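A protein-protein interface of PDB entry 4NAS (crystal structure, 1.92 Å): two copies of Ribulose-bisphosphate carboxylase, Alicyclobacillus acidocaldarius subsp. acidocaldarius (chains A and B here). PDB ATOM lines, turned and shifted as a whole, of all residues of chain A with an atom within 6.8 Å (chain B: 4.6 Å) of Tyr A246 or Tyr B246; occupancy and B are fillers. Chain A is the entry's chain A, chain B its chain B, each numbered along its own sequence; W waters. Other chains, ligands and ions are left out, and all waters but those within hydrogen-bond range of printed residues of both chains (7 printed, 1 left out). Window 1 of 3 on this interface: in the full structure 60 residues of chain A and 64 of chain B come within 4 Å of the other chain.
The side-chain hydroxyl (OG1) of Thr A90 lies close to the backbone NH (N) of Ala A92, 3.5 Å away. The backbone carbonyl oxygen (O) of Gly B219 is in hydrogen-bond range of the side-chain hydroxyl (OH) of Tyr B246, at 2.7 Å. O of Gly A219 is in hydrogen-bond range of OH of Tyr A246 (2.7 Å). The side-chain amide oxygen (OD1) of Asn A88 is in hydrogen-bond range of the side-chain hydroxyl (OG) of Ser A93 (3.0 Å). OD1 of Asn A88 lies within hydrogen-bond range of OG1 of Thr A90 (2.6 Å). The backbone carbonyl oxygen (O) of Thr A90 lies within hydrogen-bond range of the side-chain hydroxyl (OG) of Ser A93 (2.9 Å).
Water W2 lies within hydrogen-bond range of OH of Tyr B246 (2.6 Å), OG1 of Thr A90 (3.1 Å), N of Gly B219 (3.1 Å) and ND2 of Asn A88 (3.2 Å). Water W7 lies within hydrogen-bond range of the backbone carbonyl oxygen of Tyr A246 (2.6 Å), the backbone NH of Val B250 (3.1 Å) and the backbone NH of Asp B249 (3.3 Å). Water W4 lies within hydrogen-bond range of O of Tyr B246 (2.6 Å), N of Val A250 (3.0 Å) and N of Asp A249 (3.4 Å). Water W6 bridges OD2 of Asp A249 and O of Ala B245. Water W1 lies within hydrogen-bond range of N of Val A221 (3.0 Å) and O of Asp B249 (3.0 Å). Water W5 bridges the backbone NH of Tyr A248 (3.0 Å) and the backbone carbonyl oxygen of Ala B245 (3.1 Å).
Among the printed residues, pairs that only touch across the chains: Val A96 with Asn B242 (3.5 Å), Val A250 with Val B250 (3.5 Å), Tyr A246 with Tyr B246 (3.6 Å), Val A221 with Asp B249 (3.6 Å), Val A96 with Ala B245 (3.6 Å), Thr A90 with Gly B219 (3.7 Å), Asp A249 with Val B221 (3.7 Å), Tyr A246 with Ala B92 (3.7 Å), Ala A92 with Tyr B246 (3.7 Å), Val A250 with Val B221 (3.8 Å), Val A221 with Val B250 (3.9 Å), Asn A88 with Thr B218 (3.9 Å) and Phe A182 with Ala B92 (3.9 Å).
Tyr A246 touches just these residues of chain B: Ala B92 (3.7 Å) and Tyr B246 (3.6 Å). Of chain A, only Ala A92 and Tyr A246 come within 4 Å of Tyr B246. Of the printed residues of chain B, Thr A90 touches Gly B219 (3.7 Å). Printed residues of chain A within 4 Å of Val B221: Asp A249 and Val A250. Printed residues of chain B within 4 Å of Val A96: Asn B242 (3.5 Å) and Ala B245 (3.6 Å). Of the printed residues of chain B, Val A250 touches Val B221 (3.8 Å) and Val B250 (3.5 Å). Val B244 touches none of the printed residues of chain A. The nearest residue of chain B that does not touch Tyr A246 is Asp B249 (4.1 Å). The nearest residue of chain A that does not touch Tyr B246 is Gly A247 (4.1 Å).
The backbone NH (N) of Gly B219 sits close to the side-chain amide nitrogen (ND2) of Asn A88 (3.5 Å).
Ala A92 touches Tyr B246, and with the chains exchanged Tyr A246 touches Ala B92. Val A221 touches Asp B249, and with the chains exchanged Asp A249 touches Val B221. Val A221 touches Val B250, and with the chains exchanged Val A250 touches Val B221. Val B250 touches its own counterpart, Val A250. 15 positions are printed for both chains. Of the 14 pairs that touch across the chains among the printed residues, 8 have their exchanged pair printed and touching as well.
Printed residues of chain B that touch a printed residue of chain A: Ala B92, Thr B218, Gly B219, Val B221, Asn B242, Ala B245, Tyr B246, Asp B249 and Val B250. Among the printed residues, 14 pairs touch across the chains.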
ATOM      1  N   ASN A  88       0.499   0.659 -11.933  1.00  0.00           N
ATOM      2  CA  ASN A  88       0.459  -0.815 -11.861  1.00  0.00           C
ATOM      3  C   ASN A  88       1.204  -1.527 -12.987  1.00  0.00           C
ATOM      4  O   ASN A  88       0.900  -2.680 -13.275  1.00  0.00           O
ATOM      5  CB  ASN A  88      -0.990  -1.340 -11.830  1.00  0.00           C
ATOM      6  CG  ASN A  88      -1.727  -1.129 -13.179  1.00  0.00           C
ATOM      7  OD1 ASN A  88      -1.154  -0.619 -14.138  1.00  0.00           O
ATOM      8  ND2 ASN A  88      -2.983  -1.532 -13.243  1.00  0.00           N
ATOM      9  N   THR A  90       1.116  -0.857 -16.316  1.00  0.00           N
ATOM     10  CA  THR A  90       0.451  -0.834 -17.622  1.00  0.00           C
ATOM     11  C   THR A  90       0.443   0.581 -18.201  1.00  0.00           C
ATOM     12  O   THR A  90       0.499   1.558 -17.462  1.00  0.00           O
ATOM     13  CB  THR A  90      -0.996  -1.297 -17.491  1.00  0.00           C
ATOM     14  OG1 THR A  90      -1.725  -0.348 -16.704  1.00  0.00           O
ATOM     15  CG2 THR A  90      -1.057  -2.649 -16.816  1.00  0.00           C
ATOM     16  N   ALA A  92      -2.095   1.819 -19.410  1.00  0.00           N
ATOM     17  CA  ALA A  92      -3.383   2.391 -19.051  1.00  0.00           C
ATOM     18  C   ALA A  92      -3.229   3.177 -17.754  1.00  0.00           C
ATOM     19  O   ALA A  92      -3.760   4.275 -17.631  1.00  0.00           O
ATOM     20  CB  ALA A  92      -4.425   1.328 -18.925  1.00  0.00           C
ATOM     21  N   SER A  93      -2.451   2.647 -16.813  1.00  0.00           N
ATOM     22  CA  SER A  93      -2.250   3.336 -15.531  1.00  0.00           C
ATOM     23  C   SER A  93      -1.426   4.602 -15.717  1.00  0.00           C
ATOM     24  O   SER A  93      -1.667   5.627 -15.084  1.00  0.00           O
ATOM     25  CB  SER A  93      -1.586   2.415 -14.490  1.00  0.00           C
ATOM     26  OG  SER A  93      -0.194   2.211 -14.738  1.00  0.00           O
ATOM     27  N   VAL A  96      -3.823   7.255 -18.082  1.00  0.00           N
ATOM     28  CA  VAL A  96      -4.948   7.754 -17.266  1.00  0.00           C
ATOM     29  C   VAL A  96      -4.472   8.660 -16.112  1.00  0.00           C
ATOM     30  O   VAL A  96      -5.144   9.626 -15.747  1.00  0.00           O
ATOM     31  CB  VAL A  96      -5.809   6.601 -16.717  1.00  0.00           C
ATOM     32  CG1 VAL A  96      -6.767   7.081 -15.601  1.00  0.00           C
ATOM     33  CG2 VAL A  96      -6.580   5.933 -17.837  1.00  0.00           C
ATOM     34  N   PHE A 182      -6.942  -5.178 -44.342  1.00  0.00           N
ATOM     35  CA  PHE A 182      -7.720  -5.900 -43.346  1.00  0.00           C
ATOM     36  C   PHE A 182      -8.511  -7.066 -43.939  1.00  0.00           C
ATOM     37  O   PHE A 182      -8.622  -8.121 -43.309  1.00  0.00           O
ATOM     38  CB  PHE A 182      -8.652  -4.931 -42.586  1.00  0.00           C
ATOM     39  CG  PHE A 182      -7.909  -3.932 -41.765  1.00  0.00           C
ATOM     40  CD1 PHE A 182      -7.348  -4.304 -40.550  1.00  0.00           C
ATOM     41  CD2 PHE A 182      -7.718  -2.637 -42.218  1.00  0.00           C
ATOM     42  CE1 PHE A 182      -6.623  -3.401 -39.799  1.00  0.00           C
ATOM     43  CE2 PHE A 182      -7.010  -1.724 -41.464  1.00  0.00           C
ATOM     44  CZ  PHE A 182      -6.443  -2.111 -40.255  1.00  0.00           C
ATOM     45  N   ASN A 216       0.580  -7.585 -41.785  1.00  0.00           N
ATOM     46  CA  ASN A 216      -0.338  -6.811 -40.947  1.00  0.00           C
ATOM     47  C   ASN A 216      -1.000  -7.723 -39.926  1.00  0.00           C
ATOM     48  O   ASN A 216      -1.621  -8.714 -40.295  1.00  0.00           O
ATOM     49  CB  ASN A 216      -1.408  -6.130 -41.805  1.00  0.00           C
ATOM     50  CG  ASN A 216      -1.948  -4.861 -41.167  1.00  0.00           C
ATOM     51  OD1 ASN A 216      -1.413  -4.387 -40.160  1.00  0.00           O
ATOM     52  ND2 ASN A 216      -3.009  -4.304 -41.753  1.00  0.00           N
ATOM     53  N   LEU A 217      -0.833  -7.420 -38.640  1.00  0.00           N
ATOM     54  CA  LEU A 217      -1.451  -8.239 -37.604  1.00  0.00           C
ATOM     55  C   LEU A 217      -2.829  -7.678 -37.263  1.00  0.00           C
ATOM     56  O   LEU A 217      -2.951  -6.550 -36.760  1.00  0.00           O
ATOM     57  CB  LEU A 217      -0.568  -8.305 -36.352  1.00  0.00           C
ATOM     58  CG  LEU A 217      -1.185  -9.005 -35.139  1.00  0.00           C
ATOM     59  CD1 LEU A 217      -1.317 -10.529 -35.369  1.00  0.00           C
ATOM     60  CD2 LEU A 217      -0.356  -8.699 -33.888  1.00  0.00           C
ATOM     61  N   THR A 218      -3.868  -8.462 -37.540  1.00  0.00           N
ATOM     62  CA  THR A 218      -5.238  -7.942 -37.509  1.00  0.00           C
ATOM     63  C   THR A 218      -6.209  -8.915 -36.840  1.00  0.00           C
ATOM     64  O   THR A 218      -5.869 -10.086 -36.619  1.00  0.00           O
ATOM     65  CB  THR A 218      -5.744  -7.666 -38.933  1.00  0.00           C
ATOM     66  OG1 THR A 218      -5.676  -8.877 -39.700  1.00  0.00           O
ATOM     67  CG2 THR A 218      -4.885  -6.615 -39.627  1.00  0.00           C
ATOM     68  N   GLY A 219      -7.409  -8.428 -36.511  1.00  0.00           N
ATOM     69  CA  GLY A 219      -8.444  -9.280 -35.931  1.00  0.00           C
ATOM     70  C   GLY A 219      -8.833  -8.854 -34.526  1.00  0.00           C
ATOM     71  O   GLY A 219      -8.283  -7.890 -34.006  1.00  0.00           O
ATOM     72  N   PRO A 220      -9.789  -9.565 -33.896  1.00  0.00           N
ATOM     73  CA  PRO A 220     -10.169  -9.144 -32.536  1.00  0.00           C
ATOM     74  C   PRO A 220      -9.007  -9.289 -31.559  1.00  0.00           C
ATOM     75  O   PRO A 220      -8.090 -10.073 -31.793  1.00  0.00           O
ATOM     76  CB  PRO A 220     -11.291 -10.119 -32.142  1.00  0.00           C
ATOM     77  CG  PRO A 220     -11.701 -10.810 -33.434  1.00  0.00           C
ATOM     78  CD  PRO A 220     -10.494 -10.784 -34.334  1.00  0.00           C
ATOM     79  N   VAL A 221      -9.058  -8.548 -30.460  1.00  0.00           N
ATOM     80  CA  VAL A 221      -7.978  -8.558 -29.491  1.00  0.00           C
ATOM     81  C   VAL A 221      -7.803  -9.933 -28.829  1.00  0.00           C
ATOM     82  O   VAL A 221      -6.676 -10.387 -28.603  1.00  0.00           O
ATOM     83  CB  VAL A 221      -8.206  -7.471 -28.404  1.00  0.00           C
ATOM     84  CG1 VAL A 221      -7.266  -7.676 -27.225  1.00  0.00           C
ATOM     85  CG2 VAL A 221      -8.003  -6.088 -28.988  1.00  0.00           C
ATOM     86  N   LEU A 224      -5.461 -12.154 -30.931  1.00  0.00           N
ATOM     87  CA  LEU A 224      -4.304 -11.534 -31.573  1.00  0.00           C
ATOM     88  C   LEU A 224      -2.987 -12.203 -31.194  1.00  0.00           C
ATOM     89  O   LEU A 224      -2.136 -12.428 -32.055  1.00  0.00           O
ATOM     90  CB  LEU A 224      -4.242 -10.055 -31.200  1.00  0.00           C
ATOM     91  CG  LEU A 224      -3.736  -9.063 -32.237  1.00  0.00           C
ATOM     92  CD1 LEU A 224      -4.580  -9.158 -33.490  1.00  0.00           C
ATOM     93  CD2 LEU A 224      -3.828  -7.669 -31.655  1.00  0.00           C
ATOM     94  N   LEU A 240       3.597  -6.343 -38.606  1.00  0.00           N
ATOM     95  CA  LEU A 240       3.214  -4.947 -38.723  1.00  0.00           C
ATOM     96  C   LEU A 240       2.039  -4.685 -37.794  1.00  0.00           C
ATOM     97  O   LEU A 240       1.006  -5.345 -37.862  1.00  0.00           O
ATOM     98  CB  LEU A 240       2.795  -4.637 -40.156  1.00  0.00           C
ATOM     99  CG  LEU A 240       2.165  -3.284 -40.499  1.00  0.00           C
ATOM    100  CD1 LEU A 240       3.112  -2.150 -40.170  1.00  0.00           C
ATOM    101  CD2 LEU A 240       1.772  -3.240 -41.994  1.00  0.00           C
ATOM    102  N   VAL A 241       2.200  -3.729 -36.904  1.00  0.00           N
ATOM    103  CA  VAL A 241       1.165  -3.482 -35.926  1.00  0.00           C
ATOM    104  C   VAL A 241       0.764  -2.015 -35.913  1.00  0.00           C
ATOM    105  O   VAL A 241       1.610  -1.132 -35.773  1.00  0.00           O
ATOM    106  CB  VAL A 241       1.625  -3.927 -34.534  1.00  0.00           C
ATOM    107  CG1 VAL A 241       0.512  -3.710 -33.504  1.00  0.00           C
ATOM    108  CG2 VAL A 241       2.049  -5.405 -34.575  1.00  0.00           C
ATOM    109  N   ASN A 242      -0.535  -1.773 -36.092  1.00  0.00           N
ATOM    110  CA  ASN A 242      -1.126  -0.464 -35.902  1.00  0.00           C
ATOM    111  C   ASN A 242      -1.279  -0.204 -34.409  1.00  0.00           C
ATOM    112  O   ASN A 242      -2.368  -0.357 -33.852  1.00  0.00           O
ATOM    113  CB  ASN A 242      -2.483  -0.424 -36.622  1.00  0.00           C
ATOM    114  CG  ASN A 242      -2.321  -0.359 -38.139  1.00  0.00           C
ATOM    115  OD1 ASN A 242      -1.642   0.524 -38.645  1.00  0.00           O
ATOM    116  ND2 ASN A 242      -2.926  -1.303 -38.863  1.00  0.00           N
ATOM    117  N   VAL A 243      -0.168   0.155 -33.762  1.00  0.00           N
ATOM    118  CA  VAL A 243      -0.079   0.181 -32.296  1.00  0.00           C
ATOM    119  C   VAL A 243      -1.080   1.118 -31.624  1.00  0.00           C
ATOM    120  O   VAL A 243      -1.764   0.737 -30.659  1.00  0.00           O
ATOM    121  CB  VAL A 243       1.343   0.585 -31.854  1.00  0.00           C
ATOM    122  CG1 VAL A 243       1.455   0.613 -30.321  1.00  0.00           C
ATOM    123  CG2 VAL A 243       2.386  -0.369 -32.441  1.00  0.00           C
ATOM    124  N   VAL A 244      -1.160   2.352 -32.108  1.00  0.00           N
ATOM    125  CA  VAL A 244      -2.103   3.316 -31.510  1.00  0.00           C
ATOM    126  C   VAL A 244      -3.570   2.889 -31.617  1.00  0.00           C
ATOM    127  O   VAL A 244      -4.363   3.080 -30.661  1.00  0.00           O
ATOM    128  CB  VAL A 244      -1.889   4.736 -32.080  1.00  0.00           C
ATOM    129  CG1 VAL A 244      -2.900   5.696 -31.521  1.00  0.00           C
ATOM    130  CG2 VAL A 244      -0.491   5.214 -31.768  1.00  0.00           C
ATOM    131  N   ALA A 245      -3.946   2.303 -32.758  1.00  0.00           N
ATOM    132  CA  ALA A 245      -5.313   1.809 -32.968  1.00  0.00           C
ATOM    133  C   ALA A 245      -5.714   0.674 -32.013  1.00  0.00           C
ATOM    134  O   ALA A 245      -6.874   0.591 -31.573  1.00  0.00           O
ATOM    135  CB  ALA A 245      -5.511   1.327 -34.444  1.00  0.00           C
ATOM    136  N   TYR A 246      -4.785  -0.239 -31.740  1.00  0.00           N
ATOM    137  CA  TYR A 246      -5.090  -1.374 -30.855  1.00  0.00           C
ATOM    138  C   TYR A 246      -4.915  -1.025 -29.369  1.00  0.00           C
ATOM    139  O   TYR A 246      -5.588  -1.598 -28.497  1.00  0.00           O
ATOM    140  CB  TYR A 246      -4.203  -2.569 -31.199  1.00  0.00           C
ATOM    141  CG  TYR A 246      -4.805  -3.505 -32.224  1.00  0.00           C
ATOM    142  CD1 TYR A 246      -5.973  -4.206 -31.949  1.00  0.00           C
ATOM    143  CD2 TYR A 246      -4.202  -3.692 -33.456  1.00  0.00           C
ATOM    144  CE1 TYR A 246      -6.526  -5.085 -32.883  1.00  0.00           C
ATOM    145  CE2 TYR A 246      -4.748  -4.573 -34.401  1.00  0.00           C
ATOM    146  CZ  TYR A 246      -5.906  -5.255 -34.106  1.00  0.00           C
ATOM    147  OH  TYR A 246      -6.454  -6.117 -35.035  1.00  0.00           O
ATOM    148  N   GLY A 247      -4.001  -0.097 -29.090  1.00  0.00           N
ATOM    149  CA  GLY A 247      -3.676   0.296 -27.725  1.00  0.00           C
ATOM    150  C   GLY A 247      -2.300  -0.210 -27.330  1.00  0.00           C
ATOM    151  O   GLY A 247      -1.920  -1.302 -27.723  1.00  0.00           O
ATOM    152  N   TYR A 248      -1.540   0.572 -26.561  1.00  0.00           N
ATOM    153  CA  TYR A 248      -0.182   0.149 -26.239  1.00  0.00           C
ATOM    154  C   TYR A 248      -0.088  -1.108 -25.367  1.00  0.00           C
ATOM    155  O   TYR A 248       0.857  -1.886 -25.515  1.00  0.00           O
ATOM    156  CB  TYR A 248       0.622   1.251 -25.582  1.00  0.00           C
ATOM    157  CG  TYR A 248       0.835   2.492 -26.412  1.00  0.00           C
ATOM    158  CD1 TYR A 248      -0.092   3.533 -26.381  1.00  0.00           C
ATOM    159  CD2 TYR A 248       1.978   2.654 -27.175  1.00  0.00           C
ATOM    160  CE1 TYR A 248       0.112   4.691 -27.093  1.00  0.00           C
ATOM    161  CE2 TYR A 248       2.183   3.817 -27.896  1.00  0.00           C
ATOM    162  CZ  TYR A 248       1.250   4.828 -27.843  1.00  0.00           C
ATOM    163  OH  TYR A 248       1.446   5.982 -28.546  1.00  0.00           O
ATOM    164  N   ASP A 249      -1.026  -1.291 -24.441  1.00  0.00           N
ATOM    165  CA  ASP A 249      -0.996  -2.494 -23.590  1.00  0.00           C
ATOM    166  C   ASP A 249      -1.239  -3.771 -24.387  1.00  0.00           C
ATOM    167  O   ASP A 249      -0.599  -4.788 -24.134  1.00  0.00           O
ATOM    168  CB  ASP A 249      -2.002  -2.410 -22.446  1.00  0.00           C
ATOM    169  CG  ASP A 249      -1.573  -1.446 -21.377  1.00  0.00           C
ATOM    170  OD1 ASP A 249      -0.405  -1.556 -20.924  1.00  0.00           O
ATOM    171  OD2 ASP A 249      -2.407  -0.596 -20.987  1.00  0.00           O
ATOM    172  N   VAL A 250      -2.161  -3.720 -25.341  1.00  0.00           N
ATOM    173  CA  VAL A 250      -2.318  -4.841 -26.285  1.00  0.00           C
ATOM    174  C   VAL A 250      -0.960  -5.229 -26.857  1.00  0.00           C
ATOM    175  O   VAL A 250      -0.555  -6.401 -26.804  1.00  0.00           O
ATOM    176  CB  VAL A 250      -3.300  -4.483 -27.436  1.00  0.00           C
ATOM    177  CG1 VAL A 250      -3.268  -5.513 -28.542  1.00  0.00           C
ATOM    178  CG2 VAL A 250      -4.688  -4.369 -26.898  1.00  0.00           C
ATOM    179  N   VAL A 251      -0.230  -4.232 -27.347  1.00  0.00           N
ATOM    180  CA  VAL A 251       1.069  -4.473 -27.987  1.00  0.00           C
ATOM    181  C   VAL A 251       2.169  -4.895 -27.009  1.00  0.00           C
ATOM    182  O   VAL A 251       3.033  -5.713 -27.351  1.00  0.00           O
ATOM    183  CB  VAL A 251       1.501  -3.247 -28.832  1.00  0.00           C
ATOM    184  CG1 VAL A 251       2.920  -3.406 -29.388  1.00  0.00           C
ATOM    185  CG2 VAL A 251       0.524  -3.031 -29.958  1.00  0.00           C
ATOM    186  N   ALA B  92     -10.034  -1.296 -34.842  1.00  0.00           N
ATOM    187  CA  ALA B  92      -8.737  -1.094 -35.505  1.00  0.00           C
ATOM    188  C   ALA B  92      -8.891  -0.889 -37.011  1.00  0.00           C
ATOM    189  O   ALA B  92      -8.284   0.011 -37.590  1.00  0.00           O
ATOM    190  CB  ALA B  92      -7.793  -2.249 -35.233  1.00  0.00           C
ATOM    191  N   LEU B 217     -11.651  -1.440 -13.610  1.00  0.00           N
ATOM    192  CA  LEU B 217     -11.123  -2.651 -14.270  1.00  0.00           C
ATOM    193  C   LEU B 217      -9.703  -2.398 -14.729  1.00  0.00           C
ATOM    194  O   LEU B 217      -9.469  -1.527 -15.555  1.00  0.00           O
ATOM    195  CB  LEU B 217     -11.986  -3.026 -15.473  1.00  0.00           C
ATOM    196  CG  LEU B 217     -11.583  -4.306 -16.215  1.00  0.00           C
ATOM    197  CD1 LEU B 217     -11.499  -5.536 -15.287  1.00  0.00           C
ATOM    198  CD2 LEU B 217     -12.585  -4.536 -17.315  1.00  0.00           C
ATOM    199  N   THR B 218      -8.743  -3.109 -14.150  1.00  0.00           N
ATOM    200  CA  THR B 218      -7.341  -2.751 -14.333  1.00  0.00           C
ATOM    201  C   THR B 218      -6.436  -3.970 -14.445  1.00  0.00           C
ATOM    202  O   THR B 218      -6.846  -5.094 -14.141  1.00  0.00           O
ATOM    203  CB  THR B 218      -6.824  -1.933 -13.133  1.00  0.00           C
ATOM    204  OG1 THR B 218      -6.819  -2.756 -11.963  1.00  0.00           O
ATOM    205  CG2 THR B 218      -7.691  -0.734 -12.884  1.00  0.00           C
ATOM    206  N   GLY B 219      -5.186  -3.718 -14.831  1.00  0.00           N
ATOM    207  CA  GLY B 219      -4.213  -4.769 -15.050  1.00  0.00           C
ATOM    208  C   GLY B 219      -3.943  -4.984 -16.536  1.00  0.00           C
ATOM    209  O   GLY B 219      -4.483  -4.291 -17.387  1.00  0.00           O
ATOM    210  N   VAL B 221      -3.738  -6.479 -20.376  1.00  0.00           N
ATOM    211  CA  VAL B 221      -4.810  -6.837 -21.301  1.00  0.00           C
ATOM    212  C   VAL B 221      -5.136  -8.341 -21.291  1.00  0.00           C
ATOM    213  O   VAL B 221      -6.307  -8.711 -21.213  1.00  0.00           O
ATOM    214  CB  VAL B 221      -4.541  -6.307 -22.731  1.00  0.00           C
ATOM    215  CG1 VAL B 221      -5.365  -7.060 -23.759  1.00  0.00           C
ATOM    216  CG2 VAL B 221      -4.840  -4.793 -22.811  1.00  0.00           C
ATOM    217  N   LEU B 224      -7.416  -9.312 -18.548  1.00  0.00           N
ATOM    218  CA  LEU B 224      -8.517  -8.376 -18.348  1.00  0.00           C
ATOM    219  C   LEU B 224      -9.904  -9.031 -18.402  1.00  0.00           C
ATOM    220  O   LEU B 224     -10.767  -8.751 -17.572  1.00  0.00           O
ATOM    221  CB  LEU B 224      -8.434  -7.248 -19.377  1.00  0.00           C
ATOM    222  CG  LEU B 224      -9.060  -5.918 -18.967  1.00  0.00           C
ATOM    223  CD1 LEU B 224      -8.423  -5.404 -17.694  1.00  0.00           C
ATOM    224  CD2 LEU B 224      -8.898  -4.900 -20.089  1.00  0.00           C
ATOM    225  N   VAL B 241     -14.405   1.405 -16.785  1.00  0.00           N
ATOM    226  CA  VAL B 241     -13.375   1.139 -17.769  1.00  0.00           C
ATOM    227  C   VAL B 241     -12.906   2.440 -18.392  1.00  0.00           C
ATOM    228  O   VAL B 241     -13.720   3.231 -18.899  1.00  0.00           O
ATOM    229  CB  VAL B 241     -13.871   0.169 -18.881  1.00  0.00           C
ATOM    230  CG1 VAL B 241     -12.743  -0.160 -19.853  1.00  0.00           C
ATOM    231  CG2 VAL B 241     -14.390  -1.120 -18.278  1.00  0.00           C
ATOM    232  N   ASN B 242     -11.598   2.664 -18.317  1.00  0.00           N
ATOM    233  CA  ASN B 242     -10.934   3.707 -19.089  1.00  0.00           C
ATOM    234  C   ASN B 242     -10.793   3.293 -20.558  1.00  0.00           C
ATOM    235  O   ASN B 242      -9.733   2.854 -21.020  1.00  0.00           O
ATOM    236  CB  ASN B 242      -9.577   4.004 -18.491  1.00  0.00           C
ATOM    237  CG  ASN B 242      -9.696   4.631 -17.106  1.00  0.00           C
ATOM    238  OD1 ASN B 242     -10.327   5.686 -16.941  1.00  0.00           O
ATOM    239  ND2 ASN B 242      -9.124   3.969 -16.108  1.00  0.00           N
ATOM    240  N   VAL B 243     -11.880   3.453 -21.277  1.00  0.00           N
ATOM    241  CA  VAL B 243     -11.983   2.859 -22.619  1.00  0.00           C
ATOM    242  C   VAL B 243     -10.890   3.296 -23.583  1.00  0.00           C
ATOM    243  O   VAL B 243     -10.257   2.471 -24.288  1.00  0.00           O
ATOM    244  CB  VAL B 243     -13.352   3.162 -23.213  1.00  0.00           C
ATOM    245  CG1 VAL B 243     -13.490   2.476 -24.570  1.00  0.00           C
ATOM    246  CG2 VAL B 243     -14.427   2.670 -22.245  1.00  0.00           C
ATOM    247  N   VAL B 244     -10.677   4.603 -23.661  1.00  0.00           N
ATOM    248  CA  VAL B 244      -9.696   5.134 -24.608  1.00  0.00           C
ATOM    249  C   VAL B 244      -8.263   4.712 -24.243  1.00  0.00           C
ATOM    250  O   VAL B 244      -7.430   4.481 -25.127  1.00  0.00           O
ATOM    251  CB  VAL B 244      -9.814   6.693 -24.761  1.00  0.00           C
ATOM    252  CG1 VAL B 244      -8.731   7.267 -25.727  1.00  0.00           C
ATOM    253  CG2 VAL B 244     -11.215   7.074 -25.248  1.00  0.00           C
ATOM    254  N   ALA B 245      -7.964   4.598 -22.952  1.00  0.00           N
ATOM    255  CA  ALA B 245      -6.626   4.164 -22.552  1.00  0.00           C
ATOM    256  C   ALA B 245      -6.381   2.721 -23.009  1.00  0.00           C
ATOM    257  O   ALA B 245      -5.273   2.351 -23.455  1.00  0.00           O
ATOM    258  CB  ALA B 245      -6.447   4.292 -21.052  1.00  0.00           C
ATOM    259  N   TYR B 246      -7.419   1.901 -22.913  1.00  0.00           N
ATOM    260  CA  TYR B 246      -7.235   0.481 -23.203  1.00  0.00           C
ATOM    261  C   TYR B 246      -7.412   0.179 -24.687  1.00  0.00           C
ATOM    262  O   TYR B 246      -6.770  -0.726 -25.220  1.00  0.00           O
ATOM    263  CB  TYR B 246      -8.208  -0.357 -22.394  1.00  0.00           C
ATOM    264  CG  TYR B 246      -7.650  -0.811 -21.073  1.00  0.00           C
ATOM    265  CD1 TYR B 246      -6.581  -1.700 -21.023  1.00  0.00           C
ATOM    266  CD2 TYR B 246      -8.206  -0.380 -19.874  1.00  0.00           C
ATOM    267  CE1 TYR B 246      -6.070  -2.132 -19.819  1.00  0.00           C
ATOM    268  CE2 TYR B 246      -7.691  -0.815 -18.644  1.00  0.00           C
ATOM    269  CZ  TYR B 246      -6.626  -1.688 -18.632  1.00  0.00           C
ATOM    270  OH  TYR B 246      -6.122  -2.153 -17.438  1.00  0.00           O
ATOM    271  N   GLY B 247      -8.274   0.950 -25.349  1.00  0.00           N
ATOM    272  CA  GLY B 247      -8.600   0.707 -26.743  1.00  0.00           C
ATOM    273  C   GLY B 247      -9.992   0.148 -26.930  1.00  0.00           C
ATOM    274  O   GLY B 247     -10.435  -0.678 -26.134  1.00  0.00           O
ATOM    275  N   ASP B 249     -11.375  -1.971 -29.098  1.00  0.00           N
ATOM    276  CA  ASP B 249     -11.485  -3.404 -29.367  1.00  0.00           C
ATOM    277  C   ASP B 249     -11.336  -4.221 -28.105  1.00  0.00           C
ATOM    278  O   ASP B 249     -11.956  -5.276 -27.997  1.00  0.00           O
ATOM    279  CB  ASP B 249     -10.464  -3.868 -30.398  1.00  0.00           C
ATOM    280  CG  ASP B 249     -10.849  -3.479 -31.804  1.00  0.00           C
ATOM    281  OD1 ASP B 249     -12.028  -3.684 -32.175  1.00  0.00           O
ATOM    282  OD2 ASP B 249      -9.985  -2.934 -32.520  1.00  0.00           O
ATOM    283  N   VAL B 250     -10.484  -3.750 -27.188  1.00  0.00           N
ATOM    284  CA  VAL B 250     -10.314  -4.387 -25.894  1.00  0.00           C
ATOM    285  C   VAL B 250     -11.644  -4.405 -25.164  1.00  0.00           C
ATOM    286  O   VAL B 250     -12.092  -5.465 -24.706  1.00  0.00           O
ATOM    287  CB  VAL B 250      -9.288  -3.648 -24.992  1.00  0.00           C
ATOM    288  CG1 VAL B 250      -9.499  -4.034 -23.543  1.00  0.00           C
ATOM    289  CG2 VAL B 250      -7.873  -3.982 -25.384  1.00  0.00           C
HETATM  290  O   HOH W   1     -11.689  -7.235 -30.215  1.00  0.00           O
HETATM  291  O   HOH W   2      -4.647  -0.782 -15.822  1.00  0.00           O
HETATM  292  O   HOH W   3      -8.853  -0.961 -30.827  1.00  0.00           O
HETATM  293  O   HOH W   4      -4.323  -1.648 -25.063  1.00  0.00           O
HETATM  294  O   HOH W   5      -3.194   2.863 -25.636  1.00  0.00           O
HETATM  295  O   HOH W   6      -3.361   0.385 -23.249  1.00  0.00           O
HETATM  296  O   HOH W   7      -8.122  -2.093 -28.382  1.00  0.00           O
